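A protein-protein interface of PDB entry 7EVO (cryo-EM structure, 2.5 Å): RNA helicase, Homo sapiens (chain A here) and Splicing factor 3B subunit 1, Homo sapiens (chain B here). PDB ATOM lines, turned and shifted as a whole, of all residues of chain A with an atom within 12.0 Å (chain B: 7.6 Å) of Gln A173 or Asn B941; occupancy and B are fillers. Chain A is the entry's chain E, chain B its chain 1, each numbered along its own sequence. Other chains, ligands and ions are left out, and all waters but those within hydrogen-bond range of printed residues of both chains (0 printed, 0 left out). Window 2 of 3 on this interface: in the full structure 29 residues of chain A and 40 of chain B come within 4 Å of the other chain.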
ATOM      1  N   ASP A 172       2.509  10.338  18.299  1.00  0.00           N
ATOM      2  CA  ASP A 172       3.842   9.785  18.662  1.00  0.00           C
ATOM      3  C   ASP A 172       4.730   9.769  17.412  1.00  0.00           C
ATOM      4  O   ASP A 172       5.895  10.203  17.511  1.00  0.00           O
ATOM      5  CB  ASP A 172       3.710   8.394  19.287  1.00  0.00           C
ATOM      6  CG  ASP A 172       4.880   8.019  20.181  1.00  0.00           C
ATOM      7  OD1 ASP A 172       5.622   8.932  20.590  1.00  0.00           O
ATOM      8  OD2 ASP A 172       5.037   6.815  20.466  1.00  0.00           O
ATOM      9  N   GLN A 173       4.182   9.318  16.280  1.00  0.00           N
ATOM     10  CA  GLN A 173       4.948   9.258  15.006  1.00  0.00           C
ATOM     11  C   GLN A 173       5.361  10.677  14.599  1.00  0.00           C
ATOM     12  O   GLN A 173       6.516  10.852  14.172  1.00  0.00           O
ATOM     13  CB  GLN A 173       4.100   8.618  13.907  1.00  0.00           C
ATOM     14  CG  GLN A 173       4.749   8.664  12.531  1.00  0.00           C
ATOM     15  CD  GLN A 173       6.045   7.892  12.475  1.00  0.00           C
ATOM     16  OE1 GLN A 173       6.627   7.541  13.498  1.00  0.00           O
ATOM     17  NE2 GLN A 173       6.509   7.618  11.267  1.00  0.00           N
ATOM     18  N   ASN A 174       4.460  11.650  14.757  1.00  0.00           N
ATOM     19  CA  ASN A 174       4.773  13.057  14.389  1.00  0.00           C
ATOM     20  C   ASN A 174       5.929  13.549  15.266  1.00  0.00           C
ATOM     21  O   ASN A 174       6.865  14.164  14.719  1.00  0.00           O
ATOM     22  CB  ASN A 174       3.545  13.957  14.537  1.00  0.00           C
ATOM     23  CG  ASN A 174       2.382  13.510  13.677  1.00  0.00           C
ATOM     24  OD1 ASN A 174       2.579  12.957  12.597  1.00  0.00           O
ATOM     25  ND2 ASN A 174       1.168  13.744  14.147  1.00  0.00           N
ATOM     26  N   LYS A 175       5.889  13.230  16.563  1.00  0.00           N
ATOM     27  CA  LYS A 175       6.959  13.648  17.506  1.00  0.00           C
ATOM     28  C   LYS A 175       8.281  13.004  17.078  1.00  0.00           C
ATOM     29  O   LYS A 175       9.305  13.712  17.075  1.00  0.00           O
ATOM     30  CB  LYS A 175       6.596  13.226  18.933  1.00  0.00           C
ATOM     31  CG  LYS A 175       5.541  14.083  19.619  1.00  0.00           C
ATOM     32  CD  LYS A 175       4.237  14.156  18.856  1.00  0.00           C
ATOM     33  CE  LYS A 175       3.238  15.107  19.481  1.00  0.00           C
ATOM     34  NZ  LYS A 175       3.768  16.489  19.556  1.00  0.00           N
ATOM     35  N   LEU A 176       8.243  11.725  16.693  1.00  0.00           N
ATOM     36  CA  LEU A 176       9.474  11.010  16.259  1.00  0.00           C
ATOM     37  C   LEU A 176      10.037  11.688  15.004  1.00  0.00           C
ATOM     38  O   LEU A 176      11.264  11.882  14.941  1.00  0.00           O
ATOM     39  CB  LEU A 176       9.123   9.545  15.982  1.00  0.00           C
ATOM     40  CG  LEU A 176       8.738   8.724  17.210  1.00  0.00           C
ATOM     41  CD1 LEU A 176       8.402   7.294  16.820  1.00  0.00           C
ATOM     42  CD2 LEU A 176       9.851   8.744  18.244  1.00  0.00           C
ATOM     43  N   GLU A 177       9.164  12.060  14.064  1.00  0.00           N
ATOM     44  CA  GLU A 177       9.603  12.735  12.815  1.00  0.00           C
ATOM     45  C   GLU A 177      10.235  14.086  13.163  1.00  0.00           C
ATOM     46  O   GLU A 177      11.275  14.419  12.569  1.00  0.00           O
ATOM     47  CB  GLU A 177       8.421  12.891  11.859  1.00  0.00           C
ATOM     48  CG  GLU A 177       8.371  11.823  10.781  1.00  0.00           C
ATOM     49  CD  GLU A 177       8.456  10.383  11.262  1.00  0.00           C
ATOM     50  OE1 GLU A 177       8.093   9.482  10.481  1.00  0.00           O
ATOM     51  OE2 GLU A 177       8.891  10.162  12.408  1.00  0.00           O
ATOM     52  N   GLU A 178       9.639  14.814  14.111  1.00  0.00           N
ATOM     53  CA  GLU A 178      10.173  16.138  14.530  1.00  0.00           C
ATOM     54  C   GLU A 178      11.580  15.952  15.109  1.00  0.00           C
ATOM     55  O   GLU A 178      12.510  16.618  14.615  1.00  0.00           O
ATOM     56  CB  GLU A 178       9.240  16.787  15.553  1.00  0.00           C
ATOM     57  CG  GLU A 178       7.903  17.203  14.967  1.00  0.00           C
ATOM     58  CD  GLU A 178       6.882  17.677  15.987  1.00  0.00           C
ATOM     59  OE1 GLU A 178       7.228  17.732  17.183  1.00  0.00           O
ATOM     60  OE2 GLU A 178       5.743  17.988  15.584  1.00  0.00           O
ATOM     61  N   GLU A 179      11.717  15.069  16.104  1.00  0.00           N
ATOM     62  CA  GLU A 179      13.016  14.790  16.771  1.00  0.00           C
ATOM     63  C   GLU A 179      14.105  14.549  15.719  1.00  0.00           C
ATOM     64  O   GLU A 179      15.212  15.085  15.898  1.00  0.00           O
ATOM     65  CB  GLU A 179      12.885  13.576  17.693  1.00  0.00           C
ATOM     66  CG  GLU A 179      12.070  13.854  18.941  1.00  0.00           C
ATOM     67  CD  GLU A 179      12.161  12.777  20.007  1.00  0.00           C
ATOM     68  OE1 GLU A 179      12.810  11.744  19.748  1.00  0.00           O
ATOM     69  OE2 GLU A 179      11.585  12.974  21.095  1.00  0.00           O
ATOM     70  N   MET A 180      13.794  13.812  14.648  1.00  0.00           N
ATOM     71  CA  MET A 180      14.828  13.531  13.612  1.00  0.00           C
ATOM     72  C   MET A 180      15.228  14.830  12.897  1.00  0.00           C
ATOM     73  O   MET A 180      16.436  15.101  12.796  1.00  0.00           O
ATOM     74  CB  MET A 180      14.327  12.507  12.590  1.00  0.00           C
ATOM     75  CG  MET A 180      13.936  11.187  13.221  1.00  0.00           C
ATOM     76  SD  MET A 180      14.947  10.820  14.675  1.00  0.00           S
ATOM     77  CE  MET A 180      13.948   9.566  15.474  1.00  0.00           C
ATOM     78  N   ARG A 181      14.235  15.599  12.443  1.00  0.00           N
ATOM     79  CA  ARG A 181      14.428  16.882  11.716  1.00  0.00           C
ATOM     80  C   ARG A 181      15.394  17.776  12.503  1.00  0.00           C
ATOM     81  O   ARG A 181      16.379  18.248  11.909  1.00  0.00           O
ATOM     82  CB  ARG A 181      13.079  17.583  11.568  1.00  0.00           C
ATOM     83  CG  ARG A 181      13.060  18.710  10.547  1.00  0.00           C
ATOM     84  CD  ARG A 181      12.402  19.952  11.107  1.00  0.00           C
ATOM     85  NE  ARG A 181      11.379  19.652  12.099  1.00  0.00           N
ATOM     86  CZ  ARG A 181      10.971  20.498  13.040  1.00  0.00           C
ATOM     87  NH1 ARG A 181      10.030  20.122  13.895  1.00  0.00           N
ATOM     88  NH2 ARG A 181      11.495  21.713  13.139  1.00  0.00           N
ATOM     89  N   LYS A 182      15.123  17.967  13.796  1.00  0.00           N
ATOM     90  CA  LYS A 182      15.934  18.853  14.675  1.00  0.00           C
ATOM     91  C   LYS A 182      17.371  18.329  14.764  1.00  0.00           C
ATOM     92  O   LYS A 182      18.296  19.151  14.638  1.00  0.00           O
ATOM     93  CB  LYS A 182      15.294  18.962  16.059  1.00  0.00           C
ATOM     94  CG  LYS A 182      13.921  19.621  16.083  1.00  0.00           C
ATOM     95  CD  LYS A 182      13.323  19.733  17.472  1.00  0.00           C
ATOM     96  CE  LYS A 182      11.948  20.370  17.468  1.00  0.00           C
ATOM     97  NZ  LYS A 182      11.405  20.508  18.841  1.00  0.00           N
ATOM     98  N   ARG A 183      17.562  17.019  14.940  1.00  0.00           N
ATOM     99  CA  ARG A 183      18.939  16.464  15.061  1.00  0.00           C
ATOM    100  C   ARG A 183      19.711  16.755  13.767  1.00  0.00           C
ATOM    101  O   ARG A 183      20.858  17.249  13.851  1.00  0.00           O
ATOM    102  CB  ARG A 183      18.896  14.965  15.352  1.00  0.00           C
ATOM    103  CG  ARG A 183      20.239  14.273  15.180  1.00  0.00           C
ATOM    104  CD  ARG A 183      20.333  12.875  15.743  1.00  0.00           C
ATOM    105  NE  ARG A 183      20.096  12.814  17.175  1.00  0.00           N
ATOM    106  CZ  ARG A 183      19.050  12.244  17.770  1.00  0.00           C
ATOM    107  NH1 ARG A 183      18.092  11.651  17.074  1.00  0.00           N
ATOM    108  NH2 ARG A 183      18.971  12.261  19.089  1.00  0.00           N
ATOM    109  N   GLY B 934      13.684   6.235  21.032  1.00  0.00           N
ATOM    110  CA  GLY B 934      13.040   7.046  20.013  1.00  0.00           C
ATOM    111  C   GLY B 934      13.579   6.758  18.625  1.00  0.00           C
ATOM    112  O   GLY B 934      12.816   6.651  17.658  1.00  0.00           O
ATOM    113  N   THR B 935      14.901   6.611  18.511  1.00  0.00           N
ATOM    114  CA  THR B 935      15.508   6.325  17.214  1.00  0.00           C
ATOM    115  C   THR B 935      15.028   4.991  16.648  1.00  0.00           C
ATOM    116  O   THR B 935      14.657   4.903  15.469  1.00  0.00           O
ATOM    117  CB  THR B 935      17.031   6.337  17.341  1.00  0.00           C
ATOM    118  OG1 THR B 935      17.442   7.550  17.984  1.00  0.00           O
ATOM    119  CG2 THR B 935      17.683   6.256  15.972  1.00  0.00           C
ATOM    120  N   VAL B 936      15.022   3.939  17.472  1.00  0.00           N
ATOM    121  CA  VAL B 936      14.631   2.621  16.974  1.00  0.00           C
ATOM    122  C   VAL B 936      13.129   2.575  16.726  1.00  0.00           C
ATOM    123  O   VAL B 936      12.656   1.829  15.863  1.00  0.00           O
ATOM    124  CB  VAL B 936      15.082   1.502  17.934  1.00  0.00           C
ATOM    125  CG1 VAL B 936      16.590   1.314  17.870  1.00  0.00           C
ATOM    126  CG2 VAL B 936      14.598   1.737  19.350  1.00  0.00           C
ATOM    127  N   LEU B 937      12.355   3.357  17.485  1.00  0.00           N
ATOM    128  CA  LEU B 937      10.930   3.486  17.203  1.00  0.00           C
ATOM    129  C   LEU B 937      10.697   4.127  15.844  1.00  0.00           C
ATOM    130  O   LEU B 937       9.818   3.697  15.089  1.00  0.00           O
ATOM    131  CB  LEU B 937      10.249   4.298  18.306  1.00  0.00           C
ATOM    132  CG  LEU B 937       9.756   3.534  19.536  1.00  0.00           C
ATOM    133  CD1 LEU B 937       9.602   4.468  20.723  1.00  0.00           C
ATOM    134  CD2 LEU B 937       8.434   2.844  19.235  1.00  0.00           C
ATOM    135  N   TRP B 938      11.475   5.162  15.513  1.00  0.00           N
ATOM    136  CA  TRP B 938      11.322   5.792  14.204  1.00  0.00           C
ATOM    137  C   TRP B 938      11.759   4.854  13.085  1.00  0.00           C
ATOM    138  O   TRP B 938      11.142   4.828  12.014  1.00  0.00           O
ATOM    139  CB  TRP B 938      12.113   7.097  14.143  1.00  0.00           C
ATOM    140  CG  TRP B 938      12.168   7.676  12.760  1.00  0.00           C
ATOM    141  CD1 TRP B 938      11.112   8.120  12.018  1.00  0.00           C
ATOM    142  CD2 TRP B 938      13.335   7.868  11.951  1.00  0.00           C
ATOM    143  NE1 TRP B 938      11.548   8.577  10.799  1.00  0.00           N
ATOM    144  CE2 TRP B 938      12.909   8.434  10.733  1.00  0.00           C
ATOM    145  CE3 TRP B 938      14.698   7.617  12.138  1.00  0.00           C
ATOM    146  CZ2 TRP B 938      13.797   8.753   9.708  1.00  0.00           C
ATOM    147  CZ3 TRP B 938      15.577   7.935  11.118  1.00  0.00           C
ATOM    148  CH2 TRP B 938      15.124   8.497   9.919  1.00  0.00           C
ATOM    149  N   ARG B 939      12.821   4.077  13.312  1.00  0.00           N
ATOM    150  CA  ARG B 939      13.307   3.179  12.265  1.00  0.00           C
ATOM    151  C   ARG B 939      12.382   1.978  12.087  1.00  0.00           C
ATOM    152  O   ARG B 939      12.229   1.463  10.973  1.00  0.00           O
ATOM    153  CB  ARG B 939      14.728   2.711  12.583  1.00  0.00           C
ATOM    154  CG  ARG B 939      15.743   3.828  12.698  1.00  0.00           C
ATOM    155  CD  ARG B 939      16.048   4.430  11.341  1.00  0.00           C
ATOM    156  NE  ARG B 939      17.048   3.667  10.601  1.00  0.00           N
ATOM    157  CZ  ARG B 939      17.378   3.910   9.337  1.00  0.00           C
ATOM    158  NH1 ARG B 939      18.297   3.170   8.732  1.00  0.00           N
ATOM    159  NH2 ARG B 939      16.779   4.887   8.672  1.00  0.00           N
ATOM    160  N   LEU B 940      11.746   1.533  13.171  1.00  0.00           N
ATOM    161  CA  LEU B 940      10.924   0.327  13.134  1.00  0.00           C
ATOM    162  C   LEU B 940       9.502   0.632  12.679  1.00  0.00           C
ATOM    163  O   LEU B 940       8.740  -0.283  12.346  1.00  0.00           O
ATOM    164  CB  LEU B 940      10.916  -0.322  14.520  1.00  0.00           C
ATOM    165  CG  LEU B 940      10.132  -1.613  14.768  1.00  0.00           C
ATOM    166  CD1 LEU B 940      10.705  -2.773  13.976  1.00  0.00           C
ATOM    167  CD2 LEU B 940      10.091  -1.939  16.252  1.00  0.00           C
ATOM    168  N   ASN B 941       9.124   1.912  12.651  1.00  0.00           N
ATOM    169  CA  ASN B 941       7.749   2.270  12.324  1.00  0.00           C
ATOM    170  C   ASN B 941       7.383   1.943  10.882  1.00  0.00           C
ATOM    171  O   ASN B 941       6.247   1.532  10.619  1.00  0.00           O
ATOM    172  CB  ASN B 941       7.523   3.761  12.582  1.00  0.00           C
ATOM    173  CG  ASN B 941       6.626   4.019  13.774  1.00  0.00           C
ATOM    174  OD1 ASN B 941       6.696   3.318  14.784  1.00  0.00           O
ATOM    175  ND2 ASN B 941       5.775   5.031  13.663  1.00  0.00           N
ATOM    176  N   ASN B 942       8.307   2.128   9.942  1.00  0.00           N
ATOM    177  CA  ASN B 942       8.004   1.938   8.528  1.00  0.00           C
ATOM    178  C   ASN B 942       9.287   1.763   7.723  1.00  0.00           C
ATOM    179  O   ASN B 942      10.311   1.343   8.270  1.00  0.00           O
ATOM    180  CB  ASN B 942       7.168   3.097   7.987  1.00  0.00           C
ATOM    181  CG  ASN B 942       6.264   2.668   6.849  1.00  0.00           C
ATOM    182  OD1 ASN B 942       6.689   1.963   5.932  1.00  0.00           O
ATOM    183  ND2 ASN B 942       5.000   3.066   6.918  1.00  0.00           N
ATOM    184  N   LYS B 943       9.225   2.069   6.425  1.00  0.00           N
ATOM    185  CA  LYS B 943      10.352   2.006   5.495  1.00  0.00           C
ATOM    186  C   LYS B 943      10.826   0.593   5.171  1.00  0.00           C
ATOM    187  O   LYS B 943      11.962   0.221   5.485  1.00  0.00           O
ATOM    188  CB  LYS B 943      11.531   2.830   6.029  1.00  0.00           C
ATOM    189  CG  LYS B 943      11.201   4.294   6.281  1.00  0.00           C
ATOM    190  CD  LYS B 943      12.054   4.886   7.393  1.00  0.00           C
ATOM    191  CE  LYS B 943      12.169   3.940   8.578  1.00  0.00           C
ATOM    192  NZ  LYS B 943      10.884   3.763   9.304  1.00  0.00           N
ATOM    193  N   SER B 944       9.954  -0.197   4.544  1.00  0.00           N
ATOM    194  CA  SER B 944      10.306  -1.330   3.685  1.00  0.00           C
ATOM    195  C   SER B 944      10.710  -2.602   4.418  1.00  0.00           C
ATOM    196  O   SER B 944      11.033  -3.595   3.752  1.00  0.00           O
ATOM    197  CB  SER B 944      11.435  -0.965   2.708  1.00  0.00           C
ATOM    198  OG  SER B 944      12.706  -1.313   3.238  1.00  0.00           O
ATOM    199  N   VAL B 947      14.745  -1.897   6.877  1.00  0.00           N
ATOM    200  CA  VAL B 947      15.125  -1.093   8.031  1.00  0.00           C
ATOM    201  C   VAL B 947      14.476  -1.646   9.291  1.00  0.00           C
ATOM    202  O   VAL B 947      15.057  -1.601  10.382  1.00  0.00           O
ATOM    203  CB  VAL B 947      14.746   0.378   7.795  1.00  0.00           C
ATOM    204  CG1 VAL B 947      15.377   1.258   8.849  1.00  0.00           C
ATOM    205  CG2 VAL B 947      15.167   0.814   6.400  1.00  0.00           C
ATOM    206  N   ARG B 948      13.268  -2.201   9.158  1.00  0.00           N
ATOM    207  CA  ARG B 948      12.571  -2.736  10.321  1.00  0.00           C
ATOM    208  C   ARG B 948      13.261  -3.986  10.852  1.00  0.00           C
ATOM    209  O   ARG B 948      13.357  -4.174  12.069  1.00  0.00           O
ATOM    210  CB  ARG B 948      11.115  -3.038   9.973  1.00  0.00           C
ATOM    211  CG  ARG B 948      10.273  -1.807   9.686  1.00  0.00           C
ATOM    212  CD  ARG B 948       8.799  -2.163   9.579  1.00  0.00           C
ATOM    213  NE  ARG B 948       8.470  -2.697   8.261  1.00  0.00           N
ATOM    214  CZ  ARG B 948       7.247  -3.036   7.870  1.00  0.00           C
ATOM    215  NH1 ARG B 948       7.047  -3.512   6.649  1.00  0.00           N
ATOM    216  NH2 ARG B 948       6.221  -2.896   8.698  1.00  0.00           N
ATOM    217  N   ALA B 951      16.323  -2.849  12.689  1.00  0.00           N
ATOM    218  CA  ALA B 951      15.923  -2.338  13.996  1.00  0.00           C
ATOM    219  C   ALA B 951      15.576  -3.477  14.947  1.00  0.00           C
ATOM    220  O   ALA B 951      15.869  -3.409  16.147  1.00  0.00           O
ATOM    221  CB  ALA B 951      14.742  -1.381  13.844  1.00  0.00           C
ATOM    222  N   HIS B 973       6.071  -0.308  25.123  1.00  0.00           N
ATOM    223  CA  HIS B 973       5.647   0.404  23.918  1.00  0.00           C
ATOM    224  C   HIS B 973       6.257  -0.217  22.662  1.00  0.00           C
ATOM    225  O   HIS B 973       5.597  -0.317  21.622  1.00  0.00           O
ATOM    226  CB  HIS B 973       6.022   1.882  24.018  1.00  0.00           C
ATOM    227  CG  HIS B 973       5.364   2.750  22.991  1.00  0.00           C
ATOM    228  ND1 HIS B 973       4.291   2.332  22.235  1.00  0.00           N
ATOM    229  CD2 HIS B 973       5.633   4.016  22.594  1.00  0.00           C
ATOM    230  CE1 HIS B 973       3.926   3.303  21.417  1.00  0.00           C
ATOM    231  NE2 HIS B 973       4.724   4.337  21.615  1.00  0.00           N
ATOM    232  N   LEU B 974       7.522  -0.634  22.744  1.00  0.00           N
ATOM    233  CA  LEU B 974       8.175  -1.315  21.630  1.00  0.00           C
ATOM    234  C   LEU B 974       7.608  -2.712  21.418  1.00  0.00           C
ATOM    235  O   LEU B 974       7.436  -3.145  20.270  1.00  0.00           O
ATOM    236  CB  LEU B 974       9.681  -1.400  21.878  1.00  0.00           C
ATOM    237  CG  LEU B 974      10.647  -1.276  20.699  1.00  0.00           C
ATOM    238  CD1 LEU B 974      10.098  -0.359  19.626  1.00  0.00           C
ATOM    239  CD2 LEU B 974      11.997  -0.780  21.189  1.00  0.00           C
ATOM    240  N   VAL B 977       4.348  -2.655  19.411  1.00  0.00           N
ATOM    241  CA  VAL B 977       4.531  -2.456  17.976  1.00  0.00           C
ATOM    242  C   VAL B 977       5.084  -3.719  17.329  1.00  0.00           C
ATOM    243  O   VAL B 977       4.659  -4.115  16.234  1.00  0.00           O
ATOM    244  CB  VAL B 977       5.441  -1.240  17.724  1.00  0.00           C
ATOM    245  CG1 VAL B 977       5.799  -1.134  16.256  1.00  0.00           C
ATOM    246  CG2 VAL B 977       4.763   0.032  18.199  1.00  0.00           C
ATOM    247  N   TYR B 981       3.441  -6.047  14.387  1.00  0.00           N
ATOM    248  CA  TYR B 981       4.208  -6.493  13.221  1.00  0.00           C
ATOM    249  C   TYR B 981       4.417  -8.010  13.254  1.00  0.00           C
ATOM    250  O   TYR B 981       5.533  -8.515  13.159  1.00  0.00           O
ATOM    251  CB  TYR B 981       5.543  -5.758  13.149  1.00  0.00           C
ATOM    252  CG  TYR B 981       5.430  -4.317  12.716  1.00  0.00           C
ATOM    253  CD1 TYR B 981       4.587  -3.948  11.678  1.00  0.00           C
ATOM    254  CD2 TYR B 981       6.181  -3.327  13.333  1.00  0.00           C
ATOM    255  CE1 TYR B 981       4.482  -2.631  11.278  1.00  0.00           C
ATOM    256  CE2 TYR B 981       6.086  -2.009  12.936  1.00  0.00           C
ATOM    257  CZ  TYR B 981       5.236  -1.667  11.910  1.00  0.00           C
ATOM    258  OH  TYR B 981       5.139  -0.352  11.516  1.00  0.00           O
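Of the printed residues of chain B, Asp A172 touches His B973. Gln A173 touches one residue of chain B. Lys A175 touches none of the printed residues of chain B. Of the printed residues of chain B, Glu A177 touches Trp B938 (3.0 Å). Printed residues of chain A within 4 Å of Gly B934: Leu A176 and Met A180. Of chain A, only Leu A176 comes within 4 Å of Leu B937. Of the printed residues of chain A, Trp B938 touches Leu A176, Glu A177 and Met A180. No residue of chain A comes within 4 Å of Leu B940. Asn B941 touches one residue of chain A. Of the printed residues of chain A, His B973 touches Asp A172 (2.7 Å). No residue of chain A comes within 4 Å of Val B977. The nearest residue of chain B that does not touch Gln A173 is Trp B938 (4.7 Å). The nearest printed residue of chain B that does not touch Asp A172 is Leu B937 (5.1 Å).
Hydrophobic or aromatic side chains of chain B that line the printed part of chain A: Leu B937, Trp B938 and His B973. Hydrophobic or aromatic side chains of chain A that line the printed part of chain B: Leu A176 and Met A180. Among the printed residues, no Asp or Glu carboxylate lies within 4 Å of a Lys or Arg side-chain nitrogen of the other chain.
Among the printed residues, merely in contact across the chains: Leu A176 with Gly B934, Leu A176 with Leu B937, Leu A176 with Trp B938, Met A180 with Gly B934, Met A180 with Thr B935 and Met A180 with Trp B938.
The side-chain carboxylate (OD2) of Asp A172 is in hydrogen-bond range of a ring nitrogen (NE2) of His B973 (2.7 Å). The side-chain amide nitrogen of Asn B941 sits at hydrogen-bond distance from the side-chain amide oxygen of Gln A173, at 2.7 Å. The indole nitrogen (NE1) of Trp B938 sits close to the side-chain carboxylate (OE2) of Glu A177.
NE2 of Gln A173 sits at hydrogen-bond distance from OE1 of Glu A177 (2.6 Å). O of Leu B937 sits close to OD1 of Asn B941, 3.2 Å away. The side-chain amino group (NZ) of Lys B943 is in hydrogen-bond range of the backbone carbonyl oxygen (O) of Trp B938, 2.9 Å away.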
